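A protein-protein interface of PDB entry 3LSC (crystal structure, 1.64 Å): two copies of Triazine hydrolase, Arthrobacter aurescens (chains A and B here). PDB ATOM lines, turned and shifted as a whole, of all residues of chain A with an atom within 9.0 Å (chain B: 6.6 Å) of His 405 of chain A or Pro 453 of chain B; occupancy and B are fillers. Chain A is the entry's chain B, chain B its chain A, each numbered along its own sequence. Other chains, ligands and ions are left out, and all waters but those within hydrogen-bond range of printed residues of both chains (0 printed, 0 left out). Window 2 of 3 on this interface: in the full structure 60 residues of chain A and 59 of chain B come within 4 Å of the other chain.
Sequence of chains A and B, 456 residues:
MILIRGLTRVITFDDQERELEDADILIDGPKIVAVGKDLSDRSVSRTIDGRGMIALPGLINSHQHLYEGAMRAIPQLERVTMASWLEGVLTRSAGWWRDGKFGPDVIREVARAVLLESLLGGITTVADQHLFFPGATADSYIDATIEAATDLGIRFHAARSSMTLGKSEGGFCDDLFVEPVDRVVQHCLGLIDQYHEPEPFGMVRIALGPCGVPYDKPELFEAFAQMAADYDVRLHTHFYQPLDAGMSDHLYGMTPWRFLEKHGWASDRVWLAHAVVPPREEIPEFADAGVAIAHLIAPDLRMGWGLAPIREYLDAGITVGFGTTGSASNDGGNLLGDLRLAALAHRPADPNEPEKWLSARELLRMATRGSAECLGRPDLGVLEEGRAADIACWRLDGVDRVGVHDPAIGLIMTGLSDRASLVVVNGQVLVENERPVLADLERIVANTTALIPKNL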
ATOM      1  N   THR A   8     -18.009 -13.538  14.367  1.00  0.00           N
ATOM      2  CA  THR A   8     -18.360 -12.255  13.771  1.00  0.00           C
ATOM      3  C   THR A   8     -19.375 -12.416  12.647  1.00  0.00           C
ATOM      4  O   THR A   8     -20.302 -11.618  12.522  1.00  0.00           O
ATOM      5  CB  THR A   8     -17.116 -11.525  13.260  1.00  0.00           C
ATOM      6  OG1 THR A   8     -16.280 -11.222  14.380  1.00  0.00           O
ATOM      7  CG2 THR A   8     -17.513 -10.227  12.555  1.00  0.00           C
ATOM      8  N   ARG A   9     -19.203 -13.458  11.844  1.00  0.00           N
ATOM      9  CA  ARG A   9     -20.113 -13.728  10.744  1.00  0.00           C
ATOM     10  C   ARG A   9     -20.244 -15.230  10.553  1.00  0.00           C
ATOM     11  O   ARG A   9     -19.254 -15.946  10.616  1.00  0.00           O
ATOM     12  CB  ARG A   9     -19.579 -13.119   9.454  1.00  0.00           C
ATOM     13  CG  ARG A   9     -20.534 -13.224   8.283  1.00  0.00           C
ATOM     14  CD  ARG A   9     -21.834 -12.531   8.628  1.00  0.00           C
ATOM     15  NE  ARG A   9     -22.528 -12.034   7.450  1.00  0.00           N
ATOM     16  CZ  ARG A   9     -22.537 -10.765   7.062  1.00  0.00           C
ATOM     17  NH1 ARG A   9     -21.885  -9.843   7.764  1.00  0.00           N
ATOM     18  NH2 ARG A   9     -23.206 -10.416   5.973  1.00  0.00           N
ATOM     19  N   GLU A  21     -24.633 -12.445  12.368  1.00  0.00           N
ATOM     20  CA  GLU A  21     -23.554 -11.624  12.877  1.00  0.00           C
ATOM     21  C   GLU A  21     -23.501 -11.824  14.385  1.00  0.00           C
ATOM     22  O   GLU A  21     -24.544 -11.888  15.040  1.00  0.00           O
ATOM     23  CB  GLU A  21     -23.820 -10.154  12.520  1.00  0.00           C
ATOM     24  CG  GLU A  21     -22.706  -9.191  12.887  1.00  0.00           C
ATOM     25  CD  GLU A  21     -22.785  -7.907  12.083  1.00  0.00           C
ATOM     26  OE1 GLU A  21     -23.667  -7.072  12.375  1.00  0.00           O
ATOM     27  OE2 GLU A  21     -21.974  -7.736  11.147  1.00  0.00           O
ATOM     28  N   ARG A 361     -20.387 -15.140  -3.141  1.00  0.00           N
ATOM     29  CA  ARG A 361     -21.340 -16.039  -2.502  1.00  0.00           C
ATOM     30  C   ARG A 361     -21.690 -17.262  -3.352  1.00  0.00           C
ATOM     31  O   ARG A 361     -21.825 -18.367  -2.818  1.00  0.00           O
ATOM     32  CB  ARG A 361     -22.589 -15.276  -2.047  1.00  0.00           C
ATOM     33  CG  ARG A 361     -22.327 -14.502  -0.768  1.00  0.00           C
ATOM     34  CD  ARG A 361     -23.480 -13.617  -0.357  1.00  0.00           C
ATOM     35  NE  ARG A 361     -23.250 -13.072   0.977  1.00  0.00           N
ATOM     36  CZ  ARG A 361     -22.424 -12.062   1.245  1.00  0.00           C
ATOM     37  NH1 ARG A 361     -22.273 -11.643   2.493  1.00  0.00           N
ATOM     38  NH2 ARG A 361     -21.744 -11.478   0.268  1.00  0.00           N
ATOM     39  N   LEU A 396     -10.807 -12.561  10.535  1.00  0.00           N
ATOM     40  CA  LEU A 396     -11.108 -11.373   9.736  1.00  0.00           C
ATOM     41  C   LEU A 396     -10.278 -10.179  10.173  1.00  0.00           C
ATOM     42  O   LEU A 396     -10.319  -9.120   9.542  1.00  0.00           O
ATOM     43  CB  LEU A 396     -12.581 -11.015   9.902  1.00  0.00           C
ATOM     44  CG  LEU A 396     -13.584 -12.092   9.495  1.00  0.00           C
ATOM     45  CD1 LEU A 396     -14.956 -11.753  10.057  1.00  0.00           C
ATOM     46  CD2 LEU A 396     -13.625 -12.225   7.982  1.00  0.00           C
ATOM     47  N   ARG A 401      -6.707  -7.722   5.925  1.00  0.00           N
ATOM     48  CA  ARG A 401      -8.147  -7.643   5.683  1.00  0.00           C
ATOM     49  C   ARG A 401      -8.778  -6.376   6.283  1.00  0.00           C
ATOM     50  O   ARG A 401     -10.000  -6.253   6.343  1.00  0.00           O
ATOM     51  CB  ARG A 401      -8.868  -8.907   6.167  1.00  0.00           C
ATOM     52  CG  ARG A 401      -8.417 -10.189   5.447  1.00  0.00           C
ATOM     53  CD  ARG A 401      -9.353 -11.361   5.729  1.00  0.00           C
ATOM     54  NE  ARG A 401      -8.718 -12.668   5.502  1.00  0.00           N
ATOM     55  CZ  ARG A 401      -8.668 -13.282   4.325  1.00  0.00           C
ATOM     56  NH1 ARG A 401      -9.211 -12.718   3.253  1.00  0.00           N
ATOM     57  NH2 ARG A 401      -8.074 -14.468   4.223  1.00  0.00           N
ATOM     58  N   VAL A 402      -7.947  -5.428   6.696  1.00  0.00           N
ATOM     59  CA  VAL A 402      -8.478  -4.141   7.139  1.00  0.00           C
ATOM     60  C   VAL A 402      -9.202  -3.463   5.981  1.00  0.00           C
ATOM     61  O   VAL A 402      -8.755  -3.525   4.842  1.00  0.00           O
ATOM     62  CB  VAL A 402      -7.379  -3.208   7.691  1.00  0.00           C
ATOM     63  CG1 VAL A 402      -6.777  -3.791   8.953  1.00  0.00           C
ATOM     64  CG2 VAL A 402      -6.313  -2.967   6.645  1.00  0.00           C
ATOM     65  N   GLY A 403     -10.324  -2.813   6.269  1.00  0.00           N
ATOM     66  CA  GLY A 403     -11.033  -2.065   5.245  1.00  0.00           C
ATOM     67  C   GLY A 403     -12.024  -2.900   4.461  1.00  0.00           C
ATOM     68  O   GLY A 403     -12.679  -2.401   3.544  1.00  0.00           O
ATOM     69  N   VAL A 404     -12.129  -4.177   4.820  1.00  0.00           N
ATOM     70  CA  VAL A 404     -13.098  -5.073   4.196  1.00  0.00           C
ATOM     71  C   VAL A 404     -14.499  -4.763   4.713  1.00  0.00           C
ATOM     72  O   VAL A 404     -14.726  -4.727   5.918  1.00  0.00           O
ATOM     73  CB  VAL A 404     -12.762  -6.548   4.485  1.00  0.00           C
ATOM     74  CG1 VAL A 404     -13.984  -7.443   4.261  1.00  0.00           C
ATOM     75  CG2 VAL A 404     -11.578  -7.017   3.620  1.00  0.00           C
ATOM     76  N   HIS A 405     -15.442  -4.560   3.802  1.00  0.00           N
ATOM     77  CA  HIS A 405     -16.808  -4.224   4.202  1.00  0.00           C
ATOM     78  C   HIS A 405     -17.752  -5.423   4.275  1.00  0.00           C
ATOM     79  O   HIS A 405     -18.634  -5.469   5.136  1.00  0.00           O
ATOM     80  CB  HIS A 405     -17.356  -3.114   3.312  1.00  0.00           C
ATOM     81  CG  HIS A 405     -16.594  -1.836   3.448  1.00  0.00           C
ATOM     82  ND1 HIS A 405     -16.977  -0.829   4.309  1.00  0.00           N
ATOM     83  CD2 HIS A 405     -15.444  -1.421   2.867  1.00  0.00           C
ATOM     84  CE1 HIS A 405     -16.105   0.162   4.236  1.00  0.00           C
ATOM     85  NE2 HIS A 405     -15.164  -0.174   3.370  1.00  0.00           N
ATOM     86  N   ASP A 406     -17.550  -6.398   3.396  1.00  0.00           N
ATOM     87  CA  ASP A 406     -18.365  -7.606   3.387  1.00  0.00           C
ATOM     88  C   ASP A 406     -17.406  -8.775   3.554  1.00  0.00           C
ATOM     89  O   ASP A 406     -16.618  -9.056   2.654  1.00  0.00           O
ATOM     90  CB  ASP A 406     -19.136  -7.711   2.061  1.00  0.00           C
ATOM     91  CG  ASP A 406     -19.970  -8.986   1.958  1.00  0.00           C
ATOM     92  OD1 ASP A 406     -19.513 -10.048   2.419  1.00  0.00           O
ATOM     93  OD2 ASP A 406     -21.071  -8.933   1.371  1.00  0.00           O
ATOM     94  N   PRO A 407     -17.448  -9.438   4.723  1.00  0.00           N
ATOM     95  CA  PRO A 407     -16.464 -10.480   5.056  1.00  0.00           C
ATOM     96  C   PRO A 407     -16.473 -11.661   4.095  1.00  0.00           C
ATOM     97  O   PRO A 407     -15.416 -12.247   3.860  1.00  0.00           O
ATOM     98  CB  PRO A 407     -16.882 -10.936   6.461  1.00  0.00           C
ATOM     99  CG  PRO A 407     -17.730  -9.807   7.000  1.00  0.00           C
ATOM    100  CD  PRO A 407     -18.426  -9.227   5.803  1.00  0.00           C
ATOM    101  N   ALA A 408     -17.634 -12.012   3.554  1.00  0.00           N
ATOM    102  CA  ALA A 408     -17.708 -13.140   2.631  1.00  0.00           C
ATOM    103  C   ALA A 408     -16.998 -12.794   1.321  1.00  0.00           C
ATOM    104  O   ALA A 408     -16.241 -13.603   0.777  1.00  0.00           O
ATOM    105  CB  ALA A 408     -19.151 -13.538   2.385  1.00  0.00           C
ATOM    106  N   ILE A 409     -17.244 -11.592   0.813  1.00  0.00           N
ATOM    107  CA  ILE A 409     -16.543 -11.139  -0.384  1.00  0.00           C
ATOM    108  C   ILE A 409     -15.062 -11.028  -0.074  1.00  0.00           C
ATOM    109  O   ILE A 409     -14.218 -11.383  -0.895  1.00  0.00           O
ATOM    110  CB  ILE A 409     -17.077  -9.783  -0.895  1.00  0.00           C
ATOM    111  CG1 ILE A 409     -18.520  -9.933  -1.376  1.00  0.00           C
ATOM    112  CG2 ILE A 409     -16.195  -9.247  -2.034  1.00  0.00           C
ATOM    113  CD1 ILE A 409     -19.132  -8.635  -1.911  1.00  0.00           C
ATOM    114  N   GLY A 410     -14.750 -10.537   1.120  1.00  0.00           N
ATOM    115  CA  GLY A 410     -13.361 -10.364   1.525  1.00  0.00           C
ATOM    116  C   GLY A 410     -12.601 -11.682   1.583  1.00  0.00           C
ATOM    117  O   GLY A 410     -11.395 -11.730   1.353  1.00  0.00           O
ATOM    118  N   LEU A 411     -13.300 -12.767   1.886  1.00  0.00           N
ATOM    119  CA  LEU A 411     -12.633 -14.057   1.977  1.00  0.00           C
ATOM    120  C   LEU A 411     -12.044 -14.434   0.616  1.00  0.00           C
ATOM    121  O   LEU A 411     -10.969 -15.038   0.530  1.00  0.00           O
ATOM    122  CB  LEU A 411     -13.623 -15.121   2.456  1.00  0.00           C
ATOM    123  CG  LEU A 411     -13.061 -16.352   3.147  1.00  0.00           C
ATOM    124  CD1 LEU A 411     -12.126 -15.937   4.261  1.00  0.00           C
ATOM    125  CD2 LEU A 411     -14.221 -17.182   3.679  1.00  0.00           C
ATOM    126  N   THR A 414      -9.519 -10.688  -0.857  1.00  0.00           N
ATOM    127  CA  THR A 414      -8.392 -10.138  -0.099  1.00  0.00           C
ATOM    128  C   THR A 414      -7.569 -11.229   0.560  1.00  0.00           C
ATOM    129  O   THR A 414      -7.996 -12.386   0.645  1.00  0.00           O
ATOM    130  CB  THR A 414      -8.864  -9.162   1.021  1.00  0.00           C
ATOM    131  OG1 THR A 414      -9.476  -9.918   2.083  1.00  0.00           O
ATOM    132  CG2 THR A 414      -9.852  -8.144   0.456  1.00  0.00           C
ATOM    133  N   GLY B  69      -7.479   1.037   0.309  1.00  0.00           N
ATOM    134  CA  GLY B  69      -7.512   0.040   1.370  1.00  0.00           C
ATOM    135  C   GLY B  69      -8.780   0.143   2.206  1.00  0.00           C
ATOM    136  O   GLY B  69      -9.245  -0.842   2.784  1.00  0.00           O
ATOM    137  N   ALA B  70      -9.351   1.346   2.250  1.00  0.00           N
ATOM    138  CA  ALA B  70     -10.576   1.612   2.989  1.00  0.00           C
ATOM    139  C   ALA B  70     -11.834   1.214   2.214  1.00  0.00           C
ATOM    140  O   ALA B  70     -12.946   1.345   2.721  1.00  0.00           O
ATOM    141  CB  ALA B  70     -10.633   3.105   3.359  1.00  0.00           C
ATOM    142  N   MET B  71     -11.659   0.713   0.993  1.00  0.00           N
ATOM    143  CA  MET B  71     -12.785   0.464   0.096  1.00  0.00           C
ATOM    144  C   MET B  71     -12.833  -0.973  -0.423  1.00  0.00           C
ATOM    145  O   MET B  71     -13.202  -1.219  -1.570  1.00  0.00           O
ATOM    146  CB  MET B  71     -12.730   1.436  -1.078  1.00  0.00           C
ATOM    147  CG  MET B  71     -12.615   2.873  -0.630  1.00  0.00           C
ATOM    148  SD  MET B  71     -12.458   3.983  -2.034  1.00  0.00           S
ATOM    149  CE  MET B  71     -14.101   3.859  -2.705  1.00  0.00           C
ATOM    150  N   ARG B  72     -12.462  -1.915   0.428  1.00  0.00           N
ATOM    151  CA  ARG B  72     -12.401  -3.315   0.030  1.00  0.00           C
ATOM    152  C   ARG B  72     -13.744  -4.028   0.171  1.00  0.00           C
ATOM    153  O   ARG B  72     -14.486  -3.788   1.121  1.00  0.00           O
ATOM    154  CB  ARG B  72     -11.356  -4.036   0.877  1.00  0.00           C
ATOM    155  CG  ARG B  72      -9.928  -3.589   0.609  1.00  0.00           C
ATOM    156  CD  ARG B  72      -8.974  -4.152   1.636  1.00  0.00           C
ATOM    157  NE  ARG B  72      -7.639  -4.317   1.072  1.00  0.00           N
ATOM    158  CZ  ARG B  72      -6.527  -4.413   1.788  1.00  0.00           C
ATOM    159  NH1 ARG B  72      -6.570  -4.350   3.122  1.00  0.00           N
ATOM    160  NH2 ARG B  72      -5.365  -4.545   1.164  1.00  0.00           N
ATOM    161  N   ALA B  73     -14.045  -4.910  -0.780  1.00  0.00           N
ATOM    162  CA  ALA B  73     -15.169  -5.840  -0.652  1.00  0.00           C
ATOM    163  C   ALA B  73     -16.464  -5.100  -0.346  1.00  0.00           C
ATOM    164  O   ALA B  73     -17.209  -5.466   0.567  1.00  0.00           O
ATOM    165  CB  ALA B  73     -14.879  -6.873   0.433  1.00  0.00           C
ATOM    166  N   ILE B  74     -16.713  -4.037  -1.092  1.00  0.00           N
ATOM    167  CA  ILE B  74     -17.989  -3.347  -0.980  1.00  0.00           C
ATOM    168  C   ILE B  74     -18.971  -4.073  -1.885  1.00  0.00           C
ATOM    169  O   ILE B  74     -18.723  -4.215  -3.074  1.00  0.00           O
ATOM    170  CB  ILE B  74     -17.866  -1.888  -1.415  1.00  0.00           C
ATOM    171  CG1 ILE B  74     -16.944  -1.147  -0.449  1.00  0.00           C
ATOM    172  CG2 ILE B  74     -19.251  -1.251  -1.489  1.00  0.00           C
ATOM    173  CD1 ILE B  74     -16.695   0.311  -0.819  1.00  0.00           C
ATOM    174  N   PRO B  75     -20.085  -4.559  -1.319  1.00  0.00           N
ATOM    175  CA  PRO B  75     -21.030  -5.353  -2.108  1.00  0.00           C
ATOM    176  C   PRO B  75     -21.491  -4.661  -3.387  1.00  0.00           C
ATOM    177  O   PRO B  75     -21.546  -5.303  -4.430  1.00  0.00           O
ATOM    178  CB  PRO B  75     -22.203  -5.561  -1.146  1.00  0.00           C
ATOM    179  CG  PRO B  75     -21.575  -5.486   0.207  1.00  0.00           C
ATOM    180  CD  PRO B  75     -20.499  -4.446   0.087  1.00  0.00           C
ATOM    181  N   TRP B  96     -17.227  10.612   2.139  1.00  0.00           N
ATOM    182  CA  TRP B  96     -16.514  10.442   3.397  1.00  0.00           C
ATOM    183  C   TRP B  96     -15.691  11.669   3.790  1.00  0.00           C
ATOM    184  O   TRP B  96     -15.610  12.029   4.966  1.00  0.00           O
ATOM    185  CB  TRP B  96     -15.587   9.229   3.310  1.00  0.00           C
ATOM    186  CG  TRP B  96     -16.307   7.924   3.211  1.00  0.00           C
ATOM    187  CD1 TRP B  96     -17.586   7.651   3.607  1.00  0.00           C
ATOM    188  CD2 TRP B  96     -15.773   6.700   2.696  1.00  0.00           C
ATOM    189  NE1 TRP B  96     -17.884   6.322   3.365  1.00  0.00           N
ATOM    190  CE2 TRP B  96     -16.785   5.719   2.804  1.00  0.00           C
ATOM    191  CE3 TRP B  96     -14.537   6.339   2.149  1.00  0.00           C
ATOM    192  CZ2 TRP B  96     -16.597   4.400   2.385  1.00  0.00           C
ATOM    193  CZ3 TRP B  96     -14.351   5.024   1.737  1.00  0.00           C
ATOM    194  CH2 TRP B  96     -15.379   4.074   1.856  1.00  0.00           C
ATOM    195  N   LYS B 101     -14.337  12.284   7.519  1.00  0.00           N
ATOM    196  CA  LYS B 101     -13.946  10.900   7.796  1.00  0.00           C
ATOM    197  C   LYS B 101     -12.799  10.414   6.921  1.00  0.00           C
ATOM    198  O   LYS B 101     -12.404   9.246   7.011  1.00  0.00           O
ATOM    199  CB  LYS B 101     -15.134   9.967   7.569  1.00  0.00           C
ATOM    200  CG  LYS B 101     -16.255  10.104   8.579  1.00  0.00           C
ATOM    201  CD  LYS B 101     -17.485   9.373   8.087  1.00  0.00           C
ATOM    202  CE  LYS B 101     -18.387   8.974   9.232  1.00  0.00           C
ATOM    203  NZ  LYS B 101     -19.575   8.226   8.745  1.00  0.00           N
ATOM    204  N   PHE B 102     -12.272  11.284   6.073  1.00  0.00           N
ATOM    205  CA  PHE B 102     -11.326  10.842   5.054  1.00  0.00           C
ATOM    206  C   PHE B 102     -10.250  11.891   4.759  1.00  0.00           C
ATOM    207  O   PHE B 102      -9.943  12.163   3.600  1.00  0.00           O
ATOM    208  CB  PHE B 102     -12.089  10.488   3.778  1.00  0.00           C
ATOM    209  CG  PHE B 102     -11.572   9.257   3.076  1.00  0.00           C
ATOM    210  CD1 PHE B 102     -11.297   8.105   3.787  1.00  0.00           C
ATOM    211  CD2 PHE B 102     -11.382   9.261   1.704  1.00  0.00           C
ATOM    212  CE1 PHE B 102     -10.828   6.955   3.141  1.00  0.00           C
ATOM    213  CE2 PHE B 102     -10.912   8.132   1.051  1.00  0.00           C
ATOM    214  CZ  PHE B 102     -10.637   6.975   1.773  1.00  0.00           C
ATOM    215  N   VAL B 106      -6.567   9.986   8.268  1.00  0.00           N
ATOM    216  CA  VAL B 106      -7.146   8.676   7.991  1.00  0.00           C
ATOM    217  C   VAL B 106      -6.334   7.960   6.918  1.00  0.00           C
ATOM    218  O   VAL B 106      -6.019   6.769   7.051  1.00  0.00           O
ATOM    219  CB  VAL B 106      -8.620   8.794   7.555  1.00  0.00           C
ATOM    220  CG1 VAL B 106      -9.143   7.459   7.034  1.00  0.00           C
ATOM    221  CG2 VAL B 106      -9.462   9.290   8.728  1.00  0.00           C
ATOM    222  N   VAL B 110      -4.616   4.165   6.768  1.00  0.00           N
ATOM    223  CA  VAL B 110      -4.947   3.212   5.711  1.00  0.00           C
ATOM    224  C   VAL B 110      -3.660   2.805   4.990  1.00  0.00           C
ATOM    225  O   VAL B 110      -3.410   1.619   4.752  1.00  0.00           O
ATOM    226  CB  VAL B 110      -5.973   3.783   4.706  1.00  0.00           C
ATOM    227  CG1 VAL B 110      -6.178   2.827   3.534  1.00  0.00           C
ATOM    228  CG2 VAL B 110      -7.301   4.080   5.401  1.00  0.00           C
ATOM    229  N   THR B 449      -8.386   0.093  11.745  1.00  0.00           N
ATOM    230  CA  THR B 449      -9.749  -0.421  11.705  1.00  0.00           C
ATOM    231  C   THR B 449     -10.733   0.602  12.271  1.00  0.00           C
ATOM    232  O   THR B 449     -11.818   0.781  11.741  1.00  0.00           O
ATOM    233  CB  THR B 449      -9.870  -1.752  12.473  1.00  0.00           C
ATOM    234  OG1 THR B 449      -9.080  -2.756  11.811  1.00  0.00           O
ATOM    235  CG2 THR B 449     -11.323  -2.217  12.519  1.00  0.00           C
ATOM    236  N   ALA B 450     -10.324   1.276  13.340  1.00  0.00           N
ATOM    237  CA  ALA B 450     -11.141   2.304  13.994  1.00  0.00           C
ATOM    238  C   ALA B 450     -11.442   3.493  13.079  1.00  0.00           C
ATOM    239  O   ALA B 450     -12.408   4.232  13.297  1.00  0.00           O
ATOM    240  CB  ALA B 450     -10.445   2.785  15.259  1.00  0.00           C
ATOM    241  N   LEU B 451     -10.611   3.671  12.056  1.00  0.00           N
ATOM    242  CA  LEU B 451     -10.706   4.827  11.173  1.00  0.00           C
ATOM    243  C   LEU B 451     -11.385   4.554   9.827  1.00  0.00           C
ATOM    244  O   LEU B 451     -11.669   5.484   9.075  1.00  0.00           O
ATOM    245  CB  LEU B 451      -9.316   5.428  10.956  1.00  0.00           C
ATOM    246  CG  LEU B 451      -8.693   6.071  12.195  1.00  0.00           C
ATOM    247  CD1 LEU B 451      -7.257   6.509  11.939  1.00  0.00           C
ATOM    248  CD2 LEU B 451      -9.547   7.275  12.628  1.00  0.00           C
ATOM    249  N   ILE B 452     -11.655   3.289   9.517  1.00  0.00           N
ATOM    250  CA  ILE B 452     -12.331   2.963   8.266  1.00  0.00           C
ATOM    251  C   ILE B 452     -13.750   3.514   8.311  1.00  0.00           C
ATOM    252  O   ILE B 452     -14.499   3.226   9.243  1.00  0.00           O
ATOM    253  CB  ILE B 452     -12.380   1.436   8.009  1.00  0.00           C
ATOM    254  CG1 ILE B 452     -10.967   0.839   8.001  1.00  0.00           C
ATOM    255  CG2 ILE B 452     -13.090   1.135   6.702  1.00  0.00           C
ATOM    256  CD1 ILE B 452     -10.103   1.328   6.852  1.00  0.00           C
ATOM    257  N   PRO B 453     -14.123   4.326   7.313  1.00  0.00           N
ATOM    258  CA  PRO B 453     -15.465   4.919   7.346  1.00  0.00           C
ATOM    259  C   PRO B 453     -16.537   3.850   7.161  1.00  0.00           C
ATOM    260  O   PRO B 453     -16.370   2.922   6.361  1.00  0.00           O
ATOM    261  CB  PRO B 453     -15.457   5.890   6.157  1.00  0.00           C
ATOM    262  CG  PRO B 453     -14.017   6.137   5.856  1.00  0.00           C
ATOM    263  CD  PRO B 453     -13.313   4.845   6.199  1.00  0.00           C
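N of His 405 of chain A is in hydrogen-bond range of O of Arg 72 of chain B.
The backbone carbonyl oxygen of Ala 70 of chain B lies within hydrogen-bond range of a ring nitrogen (NE2) of His 405 of chain A.
O of Val 402 of chain A lies close to O of Gly 69 of chain B, 3.4 Å away.
N of Asp 406 of chain A is in hydrogen-bond range of O of Ala 73 of chain B (3.0 Å).
NH1 of Arg 72 of chain B lies within hydrogen-bond range of O of Val 402 of chain A (2.9 Å).
N of Arg 72 of chain B sits at hydrogen-bond distance from O of Gly 403 of chain A.
O of Gly 410 of chain A lies within hydrogen-bond range of NH1 of Arg 401 of chain A (3.1 Å).
The guanidinium group (NH2) of Arg 361 of chain A is in salt-bridge range of the side-chain carboxylate (OD2) of Asp 406 of chain A.
The backbone carbonyl oxygen of Gly 403 of chain A sits close to a ring nitrogen (NE2) of His 405 of chain A.
O of Gly 410 of chain A lies within hydrogen-bond range of OG1 of Thr 414 of chain A.
The backbone NH (N) of Ala 408 of chain A lies within hydrogen-bond range of the side-chain carboxylate (OD1) of Asp 406 of chain A, at 2.9 Å.
The side-chain carboxylate (OD1) of Asp 406 of chain A lies within hydrogen-bond range of the backbone NH (N) of Ile 409 of chain A (3.2 Å).
Among the printed residues, merely in contact across the chains: Gly 403 of chain A with Gly 69 of chain B, His 405 of chain A with Pro 453 of chain B, Val 404 of chain A with Arg 72 of chain B, His 405 of chain A with Ala 73 of chain B, His 405 of chain A with Ile 74 of chain B, Ile 409 of chain A with Ala 73 of chain B, Asp 406 of chain A with Pro 75 of chain B, Gly 410 of chain A with Ala 73 of chain B, Ile 409 of chain A with Pro 75 of chain B, Val 402 of chain A with Thr 449 of chain B, Gly 403 of chain A with Ala 70 of chain B, Gly 403 of chain A with Ile 452 of chain B and Val 404 of chain A with Ala 73 of chain B.
Pro 453 of chain B touches one residue of chain A.
Ala 73 of chain B touches five residues of chain A.
Printed residues of chain A within 4 Å of Thr 449 of chain B: Val 402.
Of the printed residues of chain B, Gly 410 of chain A touches Ala 73 (3.7 Å).
Of the printed residues of chain B, Val 404 of chain A touches Arg 72 (3.6 Å) and Ala 73 (3.97 Å).
Trp 96 of chain B touches none of the printed residues of chain A.
The nearest printed residue of chain A that does not touch Ile 74 of chain B is Ile 409 of chain A (4.6 Å).
Hydrophobic or aromatic side chains of chain B within 4 Å of the printed part of chain A: Ala 73, Ile 74, Pro 75 and Ile 452.
Printed residues of chain A that touch a printed residue of chain B: Val 402, Gly 403, Val 404, His 405, Asp 406, Ile 409 and Gly 410.
Hydrophobic or aromatic side chains of chain A within 4 Å of the printed part of chain B: Val 402, Val 404, His 405 and Ile 409.
Among the printed residues, no Asp or Glu carboxylate lies within 4 Å of a Lys or Arg side-chain nitrogen of the other chain.
No position is printed for both chains.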
